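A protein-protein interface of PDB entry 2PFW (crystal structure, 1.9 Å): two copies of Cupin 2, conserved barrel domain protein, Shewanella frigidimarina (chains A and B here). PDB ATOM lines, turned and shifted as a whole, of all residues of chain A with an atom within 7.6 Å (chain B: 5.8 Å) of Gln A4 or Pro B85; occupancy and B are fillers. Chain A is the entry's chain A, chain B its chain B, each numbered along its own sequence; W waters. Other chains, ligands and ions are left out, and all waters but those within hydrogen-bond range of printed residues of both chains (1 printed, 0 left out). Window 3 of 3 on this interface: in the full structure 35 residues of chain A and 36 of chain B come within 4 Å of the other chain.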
ATOM      1  N   MET A   2      28.378  34.612 -27.570  1.00  0.00           N
ATOM      2  CA  MET A   2      29.675  34.530 -26.911  1.00  0.00           C
ATOM      3  C   MET A   2      29.779  33.333 -25.977  1.00  0.00           C
ATOM      4  O   MET A   2      30.534  33.425 -25.060  1.00  0.00           O
ATOM      5  CB  MET A   2      29.998  35.817 -26.129  1.00  0.00           C
ATOM      6  CG  MET A   2      29.138  36.031 -24.877  1.00  0.00           C
ATOM      7  SD  MET A   2      29.261  37.828 -24.078  1.00  0.00           S
ATOM      8  CE  MET A   2      27.433  38.209 -24.195  1.00  0.00           C
ATOM      9  N   GLN A   3      29.019  32.276 -26.255  1.00  0.00           N
ATOM     10  CA  GLN A   3      29.153  31.039 -25.488  1.00  0.00           C
ATOM     11  C   GLN A   3      28.482  31.187 -24.126  1.00  0.00           C
ATOM     12  O   GLN A   3      27.523  30.472 -23.825  1.00  0.00           O
ATOM     13  CB  GLN A   3      30.611  30.631 -25.300  1.00  0.00           C
ATOM     14  CG  GLN A   3      31.499  30.572 -26.527  1.00  0.00           C
ATOM     15  CD  GLN A   3      31.218  29.388 -27.433  1.00  0.00           C
ATOM     16  OE1 GLN A   3      30.984  28.286 -26.938  1.00  0.00           O
ATOM     17  NE2 GLN A   3      31.229  29.620 -28.741  1.00  0.00           N
ATOM     18  N   GLN A   4      28.970  32.108 -23.296  1.00  0.00           N
ATOM     19  CA  GLN A   4      28.267  32.382 -22.039  1.00  0.00           C
ATOM     20  C   GLN A   4      28.538  33.805 -21.562  1.00  0.00           C
ATOM     21  O   GLN A   4      29.366  34.510 -22.131  1.00  0.00           O
ATOM     22  CB  GLN A   4      28.642  31.363 -20.971  1.00  0.00           C
ATOM     23  CG  GLN A   4      30.120  31.261 -20.635  1.00  0.00           C
ATOM     24  CD  GLN A   4      30.360  30.279 -19.501  1.00  0.00           C
ATOM     25  OE1 GLN A   4      29.939  29.121 -19.574  1.00  0.00           O
ATOM     26  NE2 GLN A   4      31.030  30.734 -18.449  1.00  0.00           N
ATOM     27  N   SER A   5      27.827  34.224 -20.525  1.00  0.00           N
ATOM     28  CA  SER A   5      27.970  35.578 -19.999  1.00  0.00           C
ATOM     29  C   SER A   5      28.937  35.597 -18.818  1.00  0.00           C
ATOM     30  O   SER A   5      29.238  34.543 -18.256  1.00  0.00           O
ATOM     31  CB  SER A   5      26.609  36.124 -19.563  1.00  0.00           C
ATOM     32  OG  SER A   5      26.061  35.279 -18.564  1.00  0.00           O
ATOM     33  N   GLU A   6      29.405  36.779 -18.441  1.00  0.00           N
ATOM     34  CA  GLU A   6      30.005  37.027 -17.132  1.00  0.00           C
ATOM     35  C   GLU A   6      29.182  36.361 -16.040  1.00  0.00           C
ATOM     36  O   GLU A   6      27.987  36.112 -16.221  1.00  0.00           O
ATOM     37  CB  GLU A   6      30.114  38.532 -16.897  1.00  0.00           C
ATOM     38  CG  GLU A   6      31.252  38.956 -15.988  1.00  0.00           C
ATOM     39  CD  GLU A   6      32.560  39.087 -16.746  1.00  0.00           C
ATOM     40  OE1 GLU A   6      32.480  39.307 -17.975  1.00  0.00           O
ATOM     41  OE2 GLU A   6      33.633  38.969 -16.118  1.00  0.00           O
ATOM     42  N   HIS A   7      29.796  36.057 -14.900  1.00  0.00           N
ATOM     43  CA  HIS A   7      29.066  35.442 -13.800  1.00  0.00           C
ATOM     44  C   HIS A   7      28.171  36.449 -13.081  1.00  0.00           C
ATOM     45  O   HIS A   7      27.250  36.055 -12.368  1.00  0.00           O
ATOM     46  CB  HIS A   7      30.034  34.812 -12.798  1.00  0.00           C
ATOM     47  CG  HIS A   7      30.795  33.652 -13.360  1.00  0.00           C
ATOM     48  ND1 HIS A   7      31.917  33.138 -12.748  1.00  0.00           N
ATOM     49  CD2 HIS A   7      30.605  32.901 -14.472  1.00  0.00           C
ATOM     50  CE1 HIS A   7      32.384  32.126 -13.454  1.00  0.00           C
ATOM     51  NE2 HIS A   7      31.605  31.960 -14.508  1.00  0.00           N
ATOM     52  N   GLY A  29      21.706  36.826 -18.077  1.00  0.00           N
ATOM     53  CA  GLY A  29      22.770  35.831 -18.007  1.00  0.00           C
ATOM     54  C   GLY A  29      22.441  34.630 -18.874  1.00  0.00           C
ATOM     55  O   GLY A  29      21.267  34.279 -19.013  1.00  0.00           O
ATOM     56  N   PHE A  30      23.456  34.002 -19.458  1.00  0.00           N
ATOM     57  CA  PHE A  30      23.215  32.889 -20.373  1.00  0.00           C
ATOM     58  C   PHE A  30      24.428  31.964 -20.495  1.00  0.00           C
ATOM     59  O   PHE A  30      25.557  32.414 -20.287  1.00  0.00           O
ATOM     60  CB  PHE A  30      22.832  33.424 -21.749  1.00  0.00           C
ATOM     61  CG  PHE A  30      23.961  33.983 -22.584  1.00  0.00           C
ATOM     62  CD1 PHE A  30      24.368  35.296 -22.414  1.00  0.00           C
ATOM     63  CD2 PHE A  30      24.608  33.213 -23.539  1.00  0.00           C
ATOM     64  CE1 PHE A  30      25.394  35.827 -23.172  1.00  0.00           C
ATOM     65  CE2 PHE A  30      25.644  33.729 -24.292  1.00  0.00           C
ATOM     66  CZ  PHE A  30      26.042  35.040 -24.105  1.00  0.00           C
ATOM     67  N   ASN A  31      24.203  30.704 -20.839  1.00  0.00           N
ATOM     68  CA  ASN A  31      25.100  29.837 -21.602  1.00  0.00           C
ATOM     69  C   ASN A  31      24.297  29.019 -22.612  1.00  0.00           C
ATOM     70  O   ASN A  31      23.094  29.206 -22.780  1.00  0.00           O
ATOM     71  CB  ASN A  31      25.919  28.941 -20.673  1.00  0.00           C
ATOM     72  CG  ASN A  31      25.075  27.982 -19.874  1.00  0.00           C
ATOM     73  OD1 ASN A  31      23.888  27.797 -20.134  1.00  0.00           O
ATOM     74  ND2 ASN A  31      25.677  27.343 -18.874  1.00  0.00           N
ATOM     75  N   HIS A  32      24.958  28.096 -23.289  1.00  0.00           N
ATOM     76  CA  HIS A  32      24.365  27.222 -24.278  1.00  0.00           C
ATOM     77  C   HIS A  32      23.037  26.617 -23.860  1.00  0.00           C
ATOM     78  O   HIS A  32      22.187  26.322 -24.709  1.00  0.00           O
ATOM     79  CB  HIS A  32      25.342  26.073 -24.599  1.00  0.00           C
ATOM     80  CG  HIS A  32      25.488  25.111 -23.461  1.00  0.00           C
ATOM     81  ND1 HIS A  32      26.332  25.364 -22.399  1.00  0.00           N
ATOM     82  CD2 HIS A  32      24.915  23.919 -23.196  1.00  0.00           C
ATOM     83  CE1 HIS A  32      26.271  24.368 -21.533  1.00  0.00           C
ATOM     84  NE2 HIS A  32      25.417  23.472 -21.995  1.00  0.00           N
ATOM     85  N   GLU A  33      22.775  26.386 -22.575  1.00  0.00           N
ATOM     86  CA  GLU A  33      21.572  25.616 -22.253  1.00  0.00           C
ATOM     87  C   GLU A  33      20.599  26.382 -21.372  1.00  0.00           C
ATOM     88  O   GLU A  33      19.532  25.872 -21.030  1.00  0.00           O
ATOM     89  CB  GLU A  33      21.968  24.298 -21.588  1.00  0.00           C
ATOM     90  CG  GLU A  33      22.200  24.358 -20.093  1.00  0.00           C
ATOM     91  CD  GLU A  33      22.661  23.029 -19.521  1.00  0.00           C
ATOM     92  OE1 GLU A  33      22.692  22.028 -20.269  1.00  0.00           O
ATOM     93  OE2 GLU A  33      22.993  22.990 -18.316  1.00  0.00           O
ATOM     94  N   LEU A  34      20.945  27.606 -20.990  1.00  0.00           N
ATOM     95  CA  LEU A  34      20.069  28.382 -20.110  1.00  0.00           C
ATOM     96  C   LEU A  34      20.236  29.867 -20.387  1.00  0.00           C
ATOM     97  O   LEU A  34      21.351  30.323 -20.644  1.00  0.00           O
ATOM     98  CB  LEU A  34      20.348  28.095 -18.635  1.00  0.00           C
ATOM     99  CG  LEU A  34      19.469  28.837 -17.625  1.00  0.00           C
ATOM    100  CD1 LEU A  34      18.019  28.385 -17.728  1.00  0.00           C
ATOM    101  CD2 LEU A  34      19.972  28.634 -16.203  1.00  0.00           C
ATOM    102  N   VAL A 112      22.081  36.804 -29.134  1.00  0.00           N
ATOM    103  CA  VAL A 112      23.418  37.008 -28.567  1.00  0.00           C
ATOM    104  C   VAL A 112      24.368  37.669 -29.563  1.00  0.00           C
ATOM    105  O   VAL A 112      25.567  37.740 -29.283  1.00  0.00           O
ATOM    106  CB  VAL A 112      24.019  35.684 -28.066  1.00  0.00           C
ATOM    107  CG1 VAL A 112      25.219  35.943 -27.167  1.00  0.00           C
ATOM    108  CG2 VAL A 112      22.971  34.870 -27.321  1.00  0.00           C
ATOM    109  N   HIS B  52      26.519  22.476  -8.188  1.00  0.00           N
ATOM    110  CA  HIS B  52      25.674  21.465  -8.823  1.00  0.00           C
ATOM    111  C   HIS B  52      25.806  21.539 -10.342  1.00  0.00           C
ATOM    112  O   HIS B  52      26.290  22.510 -10.928  1.00  0.00           O
ATOM    113  CB  HIS B  52      24.229  21.600  -8.363  1.00  0.00           C
ATOM    114  CG  HIS B  52      23.661  22.980  -8.390  1.00  0.00           C
ATOM    115  ND1 HIS B  52      23.797  23.839  -9.453  1.00  0.00           N
ATOM    116  CD2 HIS B  52      22.942  23.649  -7.462  1.00  0.00           C
ATOM    117  CE1 HIS B  52      23.188  24.981  -9.181  1.00  0.00           C
ATOM    118  NE2 HIS B  52      22.662  24.889  -7.976  1.00  0.00           N
ATOM    119  N   ARG B  53      25.395  20.463 -11.012  1.00  0.00           N
ATOM    120  CA  ARG B  53      25.559  20.358 -12.459  1.00  0.00           C
ATOM    121  C   ARG B  53      24.674  21.381 -13.169  1.00  0.00           C
ATOM    122  O   ARG B  53      25.067  21.958 -14.176  1.00  0.00           O
ATOM    123  CB  ARG B  53      25.207  18.952 -12.948  1.00  0.00           C
ATOM    124  CG  ARG B  53      23.767  18.538 -12.678  1.00  0.00           C
ATOM    125  CD  ARG B  53      23.555  17.074 -12.999  1.00  0.00           C
ATOM    126  NE  ARG B  53      22.194  16.608 -12.835  1.00  0.00           N
ATOM    127  CZ  ARG B  53      21.567  16.317 -11.712  1.00  0.00           C
ATOM    128  NH1 ARG B  53      22.184  16.439 -10.545  1.00  0.00           N
ATOM    129  NH2 ARG B  53      20.308  15.897 -11.758  1.00  0.00           N
ATOM    130  N   HIS B  54      23.482  21.583 -12.626  1.00  0.00           N
ATOM    131  CA  HIS B  54      22.496  22.483 -13.217  1.00  0.00           C
ATOM    132  C   HIS B  54      23.109  23.844 -13.525  1.00  0.00           C
ATOM    133  O   HIS B  54      23.807  24.427 -12.690  1.00  0.00           O
ATOM    134  CB  HIS B  54      21.309  22.661 -12.282  1.00  0.00           C
ATOM    135  CG  HIS B  54      20.724  21.417 -11.712  1.00  0.00           C
ATOM    136  ND1 HIS B  54      21.277  20.747 -10.646  1.00  0.00           N
ATOM    137  CD2 HIS B  54      19.614  20.718 -12.046  1.00  0.00           C
ATOM    138  CE1 HIS B  54      20.548  19.687 -10.345  1.00  0.00           C
ATOM    139  NE2 HIS B  54      19.530  19.647 -11.187  1.00  0.00           N
ATOM    140  N   SER B  55      22.868  24.367 -14.727  1.00  0.00           N
ATOM    141  CA  SER B  55      23.176  25.773 -14.995  1.00  0.00           C
ATOM    142  C   SER B  55      22.260  26.640 -14.134  1.00  0.00           C
ATOM    143  O   SER B  55      21.161  26.212 -13.776  1.00  0.00           O
ATOM    144  CB  SER B  55      23.023  26.091 -16.472  1.00  0.00           C
ATOM    145  OG  SER B  55      24.135  25.656 -17.231  1.00  0.00           O
ATOM    146  N   GLN B  56      22.701  27.840 -13.778  1.00  0.00           N
ATOM    147  CA  GLN B  56      21.848  28.700 -12.952  1.00  0.00           C
ATOM    148  C   GLN B  56      21.922  30.143 -13.445  1.00  0.00           C
ATOM    149  O   GLN B  56      23.009  30.686 -13.654  1.00  0.00           O
ATOM    150  CB  GLN B  56      22.218  28.630 -11.470  1.00  0.00           C
ATOM    151  CG  GLN B  56      21.354  29.516 -10.585  1.00  0.00           C
ATOM    152  CD  GLN B  56      21.593  29.360  -9.101  1.00  0.00           C
ATOM    153  OE1 GLN B  56      22.016  28.316  -8.609  1.00  0.00           O
ATOM    154  NE2 GLN B  56      21.313  30.422  -8.345  1.00  0.00           N
ATOM    155  N   VAL B  69      30.131  33.843  -6.521  1.00  0.00           N
ATOM    156  CA  VAL B  69      30.262  32.900  -7.625  1.00  0.00           C
ATOM    157  C   VAL B  69      31.739  32.640  -7.906  1.00  0.00           C
ATOM    158  O   VAL B  69      32.481  33.551  -8.272  1.00  0.00           O
ATOM    159  CB  VAL B  69      29.580  33.398  -8.911  1.00  0.00           C
ATOM    160  CG1 VAL B  69      29.750  32.385 -10.034  1.00  0.00           C
ATOM    161  CG2 VAL B  69      28.104  33.669  -8.658  1.00  0.00           C
ATOM    162  N   PHE B  83      25.064  34.536 -13.048  1.00  0.00           N
ATOM    163  CA  PHE B  83      25.119  33.267 -13.758  1.00  0.00           C
ATOM    164  C   PHE B  83      26.201  32.368 -13.154  1.00  0.00           C
ATOM    165  O   PHE B  83      27.361  32.773 -13.087  1.00  0.00           O
ATOM    166  CB  PHE B  83      25.390  33.522 -15.236  1.00  0.00           C
ATOM    167  CG  PHE B  83      25.979  32.366 -16.026  1.00  0.00           C
ATOM    168  CD1 PHE B  83      25.330  31.144 -16.085  1.00  0.00           C
ATOM    169  CD2 PHE B  83      27.176  32.527 -16.702  1.00  0.00           C
ATOM    170  CE1 PHE B  83      25.866  30.091 -16.802  1.00  0.00           C
ATOM    171  CE2 PHE B  83      27.727  31.477 -17.418  1.00  0.00           C
ATOM    172  CZ  PHE B  83      27.068  30.265 -17.459  1.00  0.00           C
ATOM    173  N   VAL B  84      25.790  31.183 -12.748  1.00  0.00           N
ATOM    174  CA  VAL B  84      26.629  30.116 -12.243  1.00  0.00           C
ATOM    175  C   VAL B  84      26.757  28.970 -13.247  1.00  0.00           C
ATOM    176  O   VAL B  84      25.812  28.200 -13.442  1.00  0.00           O
ATOM    177  CB  VAL B  84      26.045  29.525 -10.947  1.00  0.00           C
ATOM    178  CG1 VAL B  84      27.073  28.634 -10.262  1.00  0.00           C
ATOM    179  CG2 VAL B  84      25.563  30.637 -10.030  1.00  0.00           C
ATOM    180  N   PRO B  85      27.914  28.842 -13.880  1.00  0.00           N
ATOM    181  CA  PRO B  85      28.181  27.637 -14.681  1.00  0.00           C
ATOM    182  C   PRO B  85      28.016  26.379 -13.841  1.00  0.00           C
ATOM    183  O   PRO B  85      28.097  26.376 -12.610  1.00  0.00           O
ATOM    184  CB  PRO B  85      29.623  27.834 -15.146  1.00  0.00           C
ATOM    185  CG  PRO B  85      29.834  29.310 -15.096  1.00  0.00           C
ATOM    186  CD  PRO B  85      29.030  29.788 -13.914  1.00  0.00           C
ATOM    187  N   PRO B  86      27.736  25.254 -14.499  1.00  0.00           N
ATOM    188  CA  PRO B  86      27.639  23.974 -13.792  1.00  0.00           C
ATOM    189  C   PRO B  86      28.884  23.711 -12.943  1.00  0.00           C
ATOM    190  O   PRO B  86      29.981  24.031 -13.399  1.00  0.00           O
ATOM    191  CB  PRO B  86      27.562  22.965 -14.935  1.00  0.00           C
ATOM    192  CG  PRO B  86      26.902  23.726 -16.042  1.00  0.00           C
ATOM    193  CD  PRO B  86      27.467  25.121 -15.943  1.00  0.00           C
ATOM    194  N   HIS B  87      28.660  23.168 -11.764  1.00  0.00           N
ATOM    195  CA  HIS B  87      29.671  22.688 -10.839  1.00  0.00           C
ATOM    196  C   HIS B  87      30.544  23.815 -10.298  1.00  0.00           C
ATOM    197  O   HIS B  87      31.543  23.554  -9.626  1.00  0.00           O
ATOM    198  CB  HIS B  87      30.551  21.632 -11.519  1.00  0.00           C
ATOM    199  CG  HIS B  87      29.802  20.422 -11.990  1.00  0.00           C
ATOM    200  ND1 HIS B  87      29.758  20.066 -13.324  1.00  0.00           N
ATOM    201  CD2 HIS B  87      29.070  19.489 -11.343  1.00  0.00           C
ATOM    202  CE1 HIS B  87      29.036  18.971 -13.468  1.00  0.00           C
ATOM    203  NE2 HIS B  87      28.604  18.597 -12.278  1.00  0.00           N
ATOM    204  N   VAL B  88      30.186  25.066 -10.582  1.00  0.00           N
ATOM    205  CA  VAL B  88      30.941  26.187 -10.012  1.00  0.00           C
ATOM    206  C   VAL B  88      30.420  26.554  -8.625  1.00  0.00           C
ATOM    207  O   VAL B  88      29.222  26.468  -8.343  1.00  0.00           O
ATOM    208  CB  VAL B  88      30.908  27.407 -10.943  1.00  0.00           C
ATOM    209  CG1 VAL B  88      31.345  28.674 -10.221  1.00  0.00           C
ATOM    210  CG2 VAL B  88      31.794  27.171 -12.161  1.00  0.00           C
HETATM  211  O   HOH W   1      24.060  21.147 -16.647  1.00  0.00           O
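NE2 of Gln A4 touches CE2 of Phe B83, 3.5 Å away.
Gln A4 touches Pro B85.
O of Ser A5 touches CD2 of Phe B83, 3.3 Å away.
Glu A6 touches Phe B83.
ND1 of His A7 touches CG1 of Val B69 (3.6 Å).
Pro B85 touches His A7 (CG to NE2, 3.2 Å).
CE2 of Phe B83 touches O of Phe A30, 3.7 Å away.
Phe B83 touches Asn A31 (CE1 to ND2, 3.4 Å).
CD2 of Leu A34 touches O of Ser B55, 3.6 Å away.
Leu A34 touches Gln B56.
Water W1 bridges OE2 of Glu A33 (2.7 Å) and O of Arg B53 (2.8 Å).
Printed residues of chain B within 4 Å of Phe A30: Phe B83 (3.7 Å).
Printed residues of chain B within 4 Å of Asn A31: Ser B55 and Phe B83.
Of the printed residues of chain B, Leu A34 touches Ser B55 and Gln B56.
His B52 touches none of the printed residues of chain A.
Of the printed residues of chain A, Gln B56 touches Leu A34.
Printed residues of chain A within 4 Å of Phe B83: Gln A4, Ser A5, Glu A6, His A7, Phe A30 and Asn A31.
Val B84 touches none of the printed residues of chain A.
The nearest printed residue of chain B that does not touch Gln A4 is Pro B86 (5.9 Å).
O of Phe A30 is in hydrogen-bond range of N of Ser A5, 2.9 Å away.
The side-chain amide oxygen (OD1) of Asn A31 is in hydrogen-bond range of the backbone NH (N) of Glu A33 (3.0 Å).
OD1 of Asn A31 lies within hydrogen-bond range of N of Leu A34 (3.1 Å).
The backbone carbonyl oxygen (O) of Gln B56 is in hydrogen-bond range of the backbone NH (N) of Val B84, at 3.0 Å.
No position is printed for both chains.
The backbone NH of Phe B83 is in hydrogen-bond range of the backbone carbonyl oxygen of His A7, at 2.7 Å.
ND2 of Asn A31 sits at hydrogen-bond distance from OG of Ser B55 (2.8 Å).
OG of Ser B55 sits at hydrogen-bond distance from OE2 of Glu A33, 3.1 Å away.
Of the 13 printed residues of chain A, 8 touch a printed residue of chain B.
Of the 12 printed residues of chain B, 5 touch a printed residue of chain A.
Hydrophobic or aromatic side chains of chain B within 4 Å of the printed part of chain A: Val B69, Phe B83 and Pro B85.
Among the printed residues, 13 pairs touch across the chains.
Among the printed residues, no Asp or Glu carboxylate lies within 4 Å of a Lys or Arg side-chain nitrogen of the other chain.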
